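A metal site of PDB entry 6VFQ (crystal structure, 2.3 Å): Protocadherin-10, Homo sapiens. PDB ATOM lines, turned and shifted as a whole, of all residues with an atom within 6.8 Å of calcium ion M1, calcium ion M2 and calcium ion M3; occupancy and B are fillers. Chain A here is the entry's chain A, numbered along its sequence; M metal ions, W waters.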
ATOM      1  N   GLU A 116     -11.244 -17.446  -4.499  1.00  0.00           N
ATOM      2  CA  GLU A 116     -11.095 -17.477  -5.944  1.00  0.00           C
ATOM      3  C   GLU A 116     -11.822 -18.644  -6.583  1.00  0.00           C
ATOM      4  O   GLU A 116     -12.012 -18.661  -7.798  1.00  0.00           O
ATOM      5  CB  GLU A 116      -9.614 -17.499  -6.334  1.00  0.00           C
ATOM      6  CG  GLU A 116      -8.921 -18.836  -6.156  1.00  0.00           C
ATOM      7  CD  GLU A 116      -7.446 -18.820  -6.582  1.00  0.00           C
ATOM      8  OE1 GLU A 116      -7.117 -18.267  -7.650  1.00  0.00           O
ATOM      9  OE2 GLU A 116      -6.632 -19.378  -5.828  1.00  0.00           O
ATOM     10  N   LEU A 172     -12.866 -15.322 -10.388  1.00  0.00           N
ATOM     11  CA  LEU A 172     -11.681 -14.603  -9.960  1.00  0.00           C
ATOM     12  C   LEU A 172     -10.470 -15.538 -10.008  1.00  0.00           C
ATOM     13  O   LEU A 172     -10.589 -16.763  -9.965  1.00  0.00           O
ATOM     14  CB  LEU A 172     -11.862 -14.051  -8.550  1.00  0.00           C
ATOM     15  CG  LEU A 172     -13.089 -13.222  -8.223  1.00  0.00           C
ATOM     16  CD1 LEU A 172     -13.399 -13.397  -6.781  1.00  0.00           C
ATOM     17  CD2 LEU A 172     -12.815 -11.771  -8.524  1.00  0.00           C
ATOM     18  N   ASP A 173      -9.278 -14.940 -10.050  1.00  0.00           N
ATOM     19  CA  ASP A 173      -8.022 -15.685 -10.097  1.00  0.00           C
ATOM     20  C   ASP A 173      -7.027 -14.935  -9.241  1.00  0.00           C
ATOM     21  O   ASP A 173      -6.465 -13.915  -9.681  1.00  0.00           O
ATOM     22  CB  ASP A 173      -7.514 -15.833 -11.527  1.00  0.00           C
ATOM     23  CG  ASP A 173      -6.205 -16.645 -11.640  1.00  0.00           C
ATOM     24  OD1 ASP A 173      -5.807 -17.367 -10.683  1.00  0.00           O
ATOM     25  OD2 ASP A 173      -5.573 -16.553 -12.723  1.00  0.00           O
ATOM     26  N   ARG A 174      -6.782 -15.435  -8.028  1.00  0.00           N
ATOM     27  CA  ARG A 174      -5.885 -14.724  -7.116  1.00  0.00           C
ATOM     28  C   ARG A 174      -4.500 -14.586  -7.718  1.00  0.00           C
ATOM     29  O   ARG A 174      -3.815 -13.577  -7.496  1.00  0.00           O
ATOM     30  CB  ARG A 174      -5.789 -15.459  -5.794  1.00  0.00           C
ATOM     31  CG  ARG A 174      -4.987 -14.731  -4.760  1.00  0.00           C
ATOM     32  CD  ARG A 174      -4.525 -15.683  -3.667  1.00  0.00           C
ATOM     33  NE  ARG A 174      -3.473 -16.545  -4.219  1.00  0.00           N
ATOM     34  CZ  ARG A 174      -2.225 -16.140  -4.414  1.00  0.00           C
ATOM     35  NH1 ARG A 174      -1.855 -14.911  -4.073  1.00  0.00           N
ATOM     36  NH2 ARG A 174      -1.331 -16.958  -4.953  1.00  0.00           N
ATOM     37  N   GLU A 175      -4.064 -15.625  -8.445  1.00  0.00           N
ATOM     38  CA  GLU A 175      -2.743 -15.630  -9.045  1.00  0.00           C
ATOM     39  C   GLU A 175      -2.603 -14.573 -10.130  1.00  0.00           C
ATOM     40  O   GLU A 175      -1.485 -14.248 -10.530  1.00  0.00           O
ATOM     41  CB  GLU A 175      -2.454 -17.032  -9.628  1.00  0.00           C
ATOM     42  CG  GLU A 175      -2.052 -18.096  -8.588  1.00  0.00           C
ATOM     43  CD  GLU A 175      -3.180 -18.637  -7.707  1.00  0.00           C
ATOM     44  OE1 GLU A 175      -3.034 -18.565  -6.470  1.00  0.00           O
ATOM     45  OE2 GLU A 175      -4.181 -19.179  -8.225  1.00  0.00           O
ATOM     46  N   GLN A 176      -3.731 -14.036 -10.610  1.00  0.00           N
ATOM     47  CA  GLN A 176      -3.732 -12.957 -11.594  1.00  0.00           C
ATOM     48  C   GLN A 176      -3.931 -11.590 -10.967  1.00  0.00           C
ATOM     49  O   GLN A 176      -3.334 -10.609 -11.414  1.00  0.00           O
ATOM     50  CB  GLN A 176      -4.827 -13.180 -12.623  1.00  0.00           C
ATOM     51  CG  GLN A 176      -4.875 -12.119 -13.702  1.00  0.00           C
ATOM     52  CD  GLN A 176      -5.472 -12.646 -14.995  1.00  0.00           C
ATOM     53  OE1 GLN A 176      -5.752 -13.846 -15.121  1.00  0.00           O
ATOM     54  NE2 GLN A 176      -5.638 -11.756 -15.961  1.00  0.00           N
ATOM     55  N   LEU A 224      -9.177 -14.749  -1.866  1.00  0.00           N
ATOM     56  CA  LEU A 224      -8.538 -15.761  -1.034  1.00  0.00           C
ATOM     57  C   LEU A 224      -8.070 -16.936  -1.884  1.00  0.00           C
ATOM     58  O   LEU A 224      -8.764 -17.382  -2.808  1.00  0.00           O
ATOM     59  CB  LEU A 224      -9.512 -16.254   0.036  1.00  0.00           C
ATOM     60  CG  LEU A 224      -9.544 -15.417   1.303  1.00  0.00           C
ATOM     61  CD1 LEU A 224      -9.754 -13.962   1.010  1.00  0.00           C
ATOM     62  CD2 LEU A 224     -10.655 -15.952   2.211  1.00  0.00           C
ATOM     63  N   ASP A 225      -6.892 -17.461  -1.548  1.00  0.00           N
ATOM     64  CA  ASP A 225      -6.287 -18.515  -2.331  1.00  0.00           C
ATOM     65  C   ASP A 225      -7.021 -19.847  -2.193  1.00  0.00           C
ATOM     66  O   ASP A 225      -7.467 -20.230  -1.111  1.00  0.00           O
ATOM     67  CB  ASP A 225      -4.837 -18.713  -1.901  1.00  0.00           C
ATOM     68  CG  ASP A 225      -4.078 -19.663  -2.819  1.00  0.00           C
ATOM     69  OD1 ASP A 225      -4.132 -19.490  -4.057  1.00  0.00           O
ATOM     70  OD2 ASP A 225      -3.449 -20.594  -2.286  1.00  0.00           O
ATOM     71  N   SER A 226      -7.195 -20.510  -3.322  1.00  0.00           N
ATOM     72  CA  SER A 226      -7.480 -21.938  -3.373  1.00  0.00           C
ATOM     73  C   SER A 226      -6.289 -22.670  -3.971  1.00  0.00           C
ATOM     74  O   SER A 226      -5.454 -22.085  -4.669  1.00  0.00           O
ATOM     75  CB  SER A 226      -8.724 -22.229  -4.204  1.00  0.00           C
ATOM     76  OG  SER A 226      -8.410 -22.175  -5.585  1.00  0.00           O
ATOM     77  N   ASN A 227      -6.214 -23.985  -3.688  1.00  0.00           N
ATOM     78  CA  ASN A 227      -5.111 -24.805  -4.193  1.00  0.00           C
ATOM     79  C   ASN A 227      -5.466 -25.328  -5.577  1.00  0.00           C
ATOM     80  O   ASN A 227      -5.787 -26.491  -5.780  1.00  0.00           O
ATOM     81  CB  ASN A 227      -4.800 -25.952  -3.226  1.00  0.00           C
ATOM     82  CG  ASN A 227      -3.434 -26.611  -3.521  1.00  0.00           C
ATOM     83  OD1 ASN A 227      -2.600 -26.051  -4.218  1.00  0.00           O
ATOM     84  ND2 ASN A 227      -3.214 -27.798  -2.987  1.00  0.00           N
ATOM     85  N   ASP A 228      -5.420 -24.406  -6.547  1.00  0.00           N
ATOM     86  CA  ASP A 228      -5.862 -24.679  -7.908  1.00  0.00           C
ATOM     87  C   ASP A 228      -4.718 -24.737  -8.914  1.00  0.00           C
ATOM     88  O   ASP A 228      -4.967 -24.877 -10.116  1.00  0.00           O
ATOM     89  CB  ASP A 228      -6.919 -23.639  -8.326  1.00  0.00           C
ATOM     90  CG  ASP A 228      -6.421 -22.192  -8.260  1.00  0.00           C
ATOM     91  OD1 ASP A 228      -5.439 -21.870  -7.552  1.00  0.00           O
ATOM     92  OD2 ASP A 228      -7.057 -21.329  -8.923  1.00  0.00           O
ATOM     93  N   ASN A 229      -3.460 -24.649  -8.461  1.00  0.00           N
ATOM     94  CA  ASN A 229      -2.314 -24.856  -9.328  1.00  0.00           C
ATOM     95  C   ASN A 229      -1.529 -26.065  -8.850  1.00  0.00           C
ATOM     96  O   ASN A 229      -1.257 -26.211  -7.650  1.00  0.00           O
ATOM     97  CB  ASN A 229      -1.385 -23.655  -9.351  1.00  0.00           C
ATOM     98  CG  ASN A 229      -1.964 -22.514 -10.125  1.00  0.00           C
ATOM     99  OD1 ASN A 229      -1.875 -22.469 -11.353  1.00  0.00           O
ATOM    100  ND2 ASN A 229      -2.606 -21.570  -9.403  1.00  0.00           N
ATOM    101  N   VAL A 230      -1.152 -26.907  -9.815  1.00  0.00           N
ATOM    102  CA  VAL A 230      -0.378 -28.121  -9.581  1.00  0.00           C
ATOM    103  C   VAL A 230       1.081 -27.769  -9.801  1.00  0.00           C
ATOM    104  O   VAL A 230       1.386 -27.035 -10.739  1.00  0.00           O
ATOM    105  CB  VAL A 230      -0.820 -29.247 -10.525  1.00  0.00           C
ATOM    106  CG1 VAL A 230       0.102 -30.479 -10.385  1.00  0.00           C
ATOM    107  CG2 VAL A 230      -2.301 -29.569 -10.258  1.00  0.00           C
ATOM    108  N   PRO A 231       2.008 -28.267  -8.979  1.00  0.00           N
ATOM    109  CA  PRO A 231       3.427 -28.024  -9.244  1.00  0.00           C
ATOM    110  C   PRO A 231       3.800 -28.482 -10.650  1.00  0.00           C
ATOM    111  O   PRO A 231       3.258 -29.442 -11.187  1.00  0.00           O
ATOM    112  CB  PRO A 231       4.138 -28.851  -8.175  1.00  0.00           C
ATOM    113  CG  PRO A 231       3.145 -28.928  -7.056  1.00  0.00           C
ATOM    114  CD  PRO A 231       1.806 -29.017  -7.719  1.00  0.00           C
ATOM    115  N   ASP A 259       5.016 -23.583  -8.277  1.00  0.00           N
ATOM    116  CA  ASP A 259       3.627 -23.614  -7.817  1.00  0.00           C
ATOM    117  C   ASP A 259       3.277 -22.203  -7.364  1.00  0.00           C
ATOM    118  O   ASP A 259       3.737 -21.758  -6.313  1.00  0.00           O
ATOM    119  CB  ASP A 259       3.465 -24.624  -6.682  1.00  0.00           C
ATOM    120  CG  ASP A 259       1.998 -24.938  -6.372  1.00  0.00           C
ATOM    121  OD1 ASP A 259       1.133 -24.026  -6.327  1.00  0.00           O
ATOM    122  OD2 ASP A 259       1.698 -26.133  -6.137  1.00  0.00           O
ATOM    123  N   PRO A 260       2.482 -21.463  -8.133  1.00  0.00           N
ATOM    124  CA  PRO A 260       2.193 -20.064  -7.775  1.00  0.00           C
ATOM    125  C   PRO A 260       1.176 -19.864  -6.647  1.00  0.00           C
ATOM    126  O   PRO A 260       0.925 -18.710  -6.286  1.00  0.00           O
ATOM    127  CB  PRO A 260       1.659 -19.483  -9.074  1.00  0.00           C
ATOM    128  CG  PRO A 260       1.053 -20.668  -9.783  1.00  0.00           C
ATOM    129  CD  PRO A 260       1.901 -21.839  -9.433  1.00  0.00           C
ATOM    130  N   ASP A 261       0.592 -20.914  -6.060  1.00  0.00           N
ATOM    131  CA  ASP A 261      -0.382 -20.714  -5.001  1.00  0.00           C
ATOM    132  C   ASP A 261       0.273 -20.071  -3.791  1.00  0.00           C
ATOM    133  O   ASP A 261       1.477 -19.829  -3.765  1.00  0.00           O
ATOM    134  CB  ASP A 261      -1.053 -22.033  -4.628  1.00  0.00           C
ATOM    135  CG  ASP A 261      -1.963 -22.546  -5.716  1.00  0.00           C
ATOM    136  OD1 ASP A 261      -2.636 -21.720  -6.353  1.00  0.00           O
ATOM    137  OD2 ASP A 261      -1.985 -23.777  -5.956  1.00  0.00           O
ATOM    138  N   GLU A 262      -0.527 -19.816  -2.763  1.00  0.00           N
ATOM    139  CA  GLU A 262      -0.105 -19.105  -1.563  1.00  0.00           C
ATOM    140  C   GLU A 262      -0.015 -20.069  -0.374  1.00  0.00           C
ATOM    141  O   GLU A 262      -0.716 -21.074  -0.327  1.00  0.00           O
ATOM    142  CB  GLU A 262      -1.108 -17.981  -1.270  1.00  0.00           C
ATOM    143  CG  GLU A 262      -0.915 -17.223   0.006  1.00  0.00           C
ATOM    144  CD  GLU A 262      -2.001 -16.161   0.189  1.00  0.00           C
ATOM    145  OE1 GLU A 262      -1.793 -15.020  -0.259  1.00  0.00           O
ATOM    146  OE2 GLU A 262      -3.073 -16.487   0.758  1.00  0.00           O
ATOM    147  N   GLN A 264       0.832 -22.940   2.298  1.00  0.00           N
ATOM    148  CA  GLN A 264       1.058 -24.368   2.108  1.00  0.00           C
ATOM    149  C   GLN A 264       0.629 -24.817   0.714  1.00  0.00           C
ATOM    150  O   GLN A 264       1.263 -25.692   0.120  1.00  0.00           O
ATOM    151  CB  GLN A 264       0.305 -25.150   3.190  1.00  0.00           C
ATOM    152  CG  GLN A 264       0.777 -24.849   4.625  1.00  0.00           C
ATOM    153  CD  GLN A 264       2.289 -24.964   4.792  1.00  0.00           C
ATOM    154  OE1 GLN A 264       2.850 -26.069   4.928  1.00  0.00           O
ATOM    155  NE2 GLN A 264       2.970 -23.819   4.734  1.00  0.00           N
ATOM    156  N   ASN A 265      -0.438 -24.208   0.161  1.00  0.00           N
ATOM    157  CA  ASN A 265      -0.869 -24.529  -1.193  1.00  0.00           C
ATOM    158  C   ASN A 265       0.261 -24.377  -2.187  1.00  0.00           C
ATOM    159  O   ASN A 265       0.253 -25.024  -3.239  1.00  0.00           O
ATOM    160  CB  ASN A 265      -2.031 -23.633  -1.633  1.00  0.00           C
ATOM    161  CG  ASN A 265      -3.238 -23.800  -0.770  1.00  0.00           C
ATOM    162  OD1 ASN A 265      -3.405 -24.829  -0.130  1.00  0.00           O
ATOM    163  ND2 ASN A 265      -4.089 -22.779  -0.733  1.00  0.00           N
ATOM    164  N   GLY A 266       1.212 -23.501  -1.884  1.00  0.00           N
ATOM    165  CA  GLY A 266       2.267 -23.207  -2.824  1.00  0.00           C
ATOM    166  C   GLY A 266       3.635 -23.731  -2.424  1.00  0.00           C
ATOM    167  O   GLY A 266       4.602 -23.519  -3.154  1.00  0.00           O
ATOM    168  N   GLU A 267       3.724 -24.390  -1.266  1.00  0.00           N
ATOM    169  CA  GLU A 267       4.975 -24.982  -0.804  1.00  0.00           C
ATOM    170  C   GLU A 267       5.100 -26.405  -1.326  1.00  0.00           C
ATOM    171  O   GLU A 267       4.192 -27.227  -1.131  1.00  0.00           O
ATOM    172  CB  GLU A 267       5.044 -24.986   0.733  1.00  0.00           C
ATOM    173  CG  GLU A 267       5.361 -23.652   1.373  1.00  0.00           C
ATOM    174  CD  GLU A 267       6.738 -23.117   0.988  1.00  0.00           C
ATOM    175  OE1 GLU A 267       7.714 -23.906   0.928  1.00  0.00           O
ATOM    176  OE2 GLU A 267       6.834 -21.897   0.729  1.00  0.00           O
ATOM    177  N   VAL A 268       6.230 -26.699  -1.986  1.00  0.00           N
ATOM    178  CA  VAL A 268       6.431 -27.947  -2.708  1.00  0.00           C
ATOM    179  C   VAL A 268       7.483 -28.795  -1.986  1.00  0.00           C
ATOM    180  O   VAL A 268       8.551 -28.302  -1.604  1.00  0.00           O
ATOM    181  CB  VAL A 268       6.878 -27.674  -4.157  1.00  0.00           C
ATOM    182  CG1 VAL A 268       7.092 -28.973  -4.888  1.00  0.00           C
ATOM    183  CG2 VAL A 268       5.863 -26.851  -4.851  1.00  0.00           C
ATOM    184  N   ASP A 315       2.497 -30.254  -3.607  1.00  0.00           N
ATOM    185  CA  ASP A 315       2.461 -29.153  -2.657  1.00  0.00           C
ATOM    186  C   ASP A 315       1.890 -29.663  -1.331  1.00  0.00           C
ATOM    187  O   ASP A 315       1.479 -30.816  -1.215  1.00  0.00           O
ATOM    188  CB  ASP A 315       1.715 -27.950  -3.227  1.00  0.00           C
ATOM    189  CG  ASP A 315       0.213 -28.188  -3.463  1.00  0.00           C
ATOM    190  OD1 ASP A 315      -0.500 -28.654  -2.547  1.00  0.00           O
ATOM    191  OD2 ASP A 315      -0.254 -27.883  -4.586  1.00  0.00           O
ATOM    192  N   LEU A 316       1.924 -28.803  -0.320  1.00  0.00           N
ATOM    193  CA  LEU A 316       1.509 -29.161   1.020  1.00  0.00           C
ATOM    194  C   LEU A 316       0.066 -28.749   1.349  1.00  0.00           C
ATOM    195  O   LEU A 316      -0.336 -28.774   2.521  1.00  0.00           O
ATOM    196  CB  LEU A 316       2.477 -28.549   2.021  1.00  0.00           C
ATOM    197  CG  LEU A 316       3.900 -29.109   2.016  1.00  0.00           C
ATOM    198  CD1 LEU A 316       4.822 -28.269   2.867  1.00  0.00           C
ATOM    199  CD2 LEU A 316       3.942 -30.508   2.520  1.00  0.00           C
ATOM    200  N   GLY A 317      -0.739 -28.385   0.351  1.00  0.00           N
ATOM    201  CA  GLY A 317      -2.108 -27.959   0.604  1.00  0.00           C
ATOM    202  C   GLY A 317      -3.103 -29.116   0.568  1.00  0.00           C
ATOM    203  O   GLY A 317      -2.758 -30.256   0.247  1.00  0.00           O
ATOM    204  N   ALA A 320      -3.994 -31.773  -2.726  1.00  0.00           N
ATOM    205  CA  ALA A 320      -2.836 -31.615  -3.598  1.00  0.00           C
ATOM    206  C   ALA A 320      -2.794 -32.710  -4.648  1.00  0.00           C
ATOM    207  O   ALA A 320      -3.165 -33.859  -4.407  1.00  0.00           O
ATOM    208  CB  ALA A 320      -1.555 -31.627  -2.770  1.00  0.00           C
HETATM  209 CA    CA M   1      -0.600 -25.676  -5.436  1.00  0.00          CA
HETATM  210 CA    CA M   2      -4.522 -20.373  -6.066  1.00  0.00          CA
HETATM  211 CA    CA M   3      -6.190 -19.314  -9.536  1.00  0.00          CA
HETATM  212  O   HOH W   1      -4.851 -20.630 -11.009  1.00  0.00           O
HETATM  213  O   HOH W   2      -7.869 -18.907 -11.111  1.00  0.00           O
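The side-chain carboxylate of Asp 225 sits at hydrogen-bond distance from the side-chain amide nitrogen of Asn 265 (2.8 Å). The side-chain carboxylate (OD1) of Asp 225 sits close to the guanidinium group (NE) of Arg 174. OD2 of Asp 225 is in hydrogen-bond range of N of Glu 262 (3.1 Å). The side-chain carboxylate (OE1) of Glu 116 sits close to the backbone NH (N) of Arg 174 (2.9 Å). O of Leu 224 lies within hydrogen-bond range of N of Glu 116. The side-chain amide nitrogen (ND2) of Asn 229 sits close to the side-chain carboxylate (OE2) of Glu 175 (3.1 Å). OE1 of Glu 175 sits close to NH2 of Arg 174, 2.8 Å away. N of Gly 317 lies within hydrogen-bond range of OD1 of Asp 315, at 2.9 Å.
Six residues have an atom within 4 Å of calcium ion M1: Asn 227, Asn 229, Asp 259, Asp 261, Asn 265 and Asp 315.
Of the 27 residues printed, 6 come within 4 Å of calcium ion M2. Along chain A the residues within 4 Å of calcium ion M2 span positions 116 to 261. The nearest printed residue that does not touch calcium ion M2 is Asn 229 (4.03 Å).
Within 4 Å of calcium ion M3: Glu 116, Asp 173, Glu 175 and Asp 228. The nearest printed residue that does not touch calcium ion M3 is Arg 174 (4.2 Å).
Calcium ion M1 is bound by O of Asn 229 (2.4 Å), OD1 of Asn 227 (2.4 Å), OD2 of Asp 315 (2.4 Å), OD2 of Asp 261 (2.4 Å), O of Asn 265 (2.4 Å), OD2 of Asp 259 (2.4 Å) and OD1 of Asp 259 (2.6 Å). Calcium ion M1 has seven donor atoms within binding distance.
OD1 of Asp 225 binds calcium ion M2, at 2.2 Å. OD1 of Asp 228 binds calcium ion M2 (2.3 Å). OD1 of Asp 261 binds calcium ion M2 (2.3 Å). OE2 of Glu 116 binds calcium ion M2 (2.3 Å). Calcium ion M2 is bound by OE1 of Glu 175 (2.4 Å). Calcium ion M2 is bound by the backbone carbonyl oxygen (O) of Ser 226 (2.4 Å). OE2 of Glu 175 binds calcium ion M2 (2.5 Å).
Calcium ion M3 is bound by OD2 of Asp 228, 2.3 Å away. OD1 of Asp 173 binds calcium ion M3 (2.3 Å). Water W2 binds calcium ion M3, 2.3 Å away. Calcium ion M3 is bound by the side-chain carboxylate (OE1) of Glu 116 (2.3 Å). Water W1 binds calcium ion M3 (2.4 Å). Calcium ion M3 is bound by OE2 of Glu 175, at 2.4 Å.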
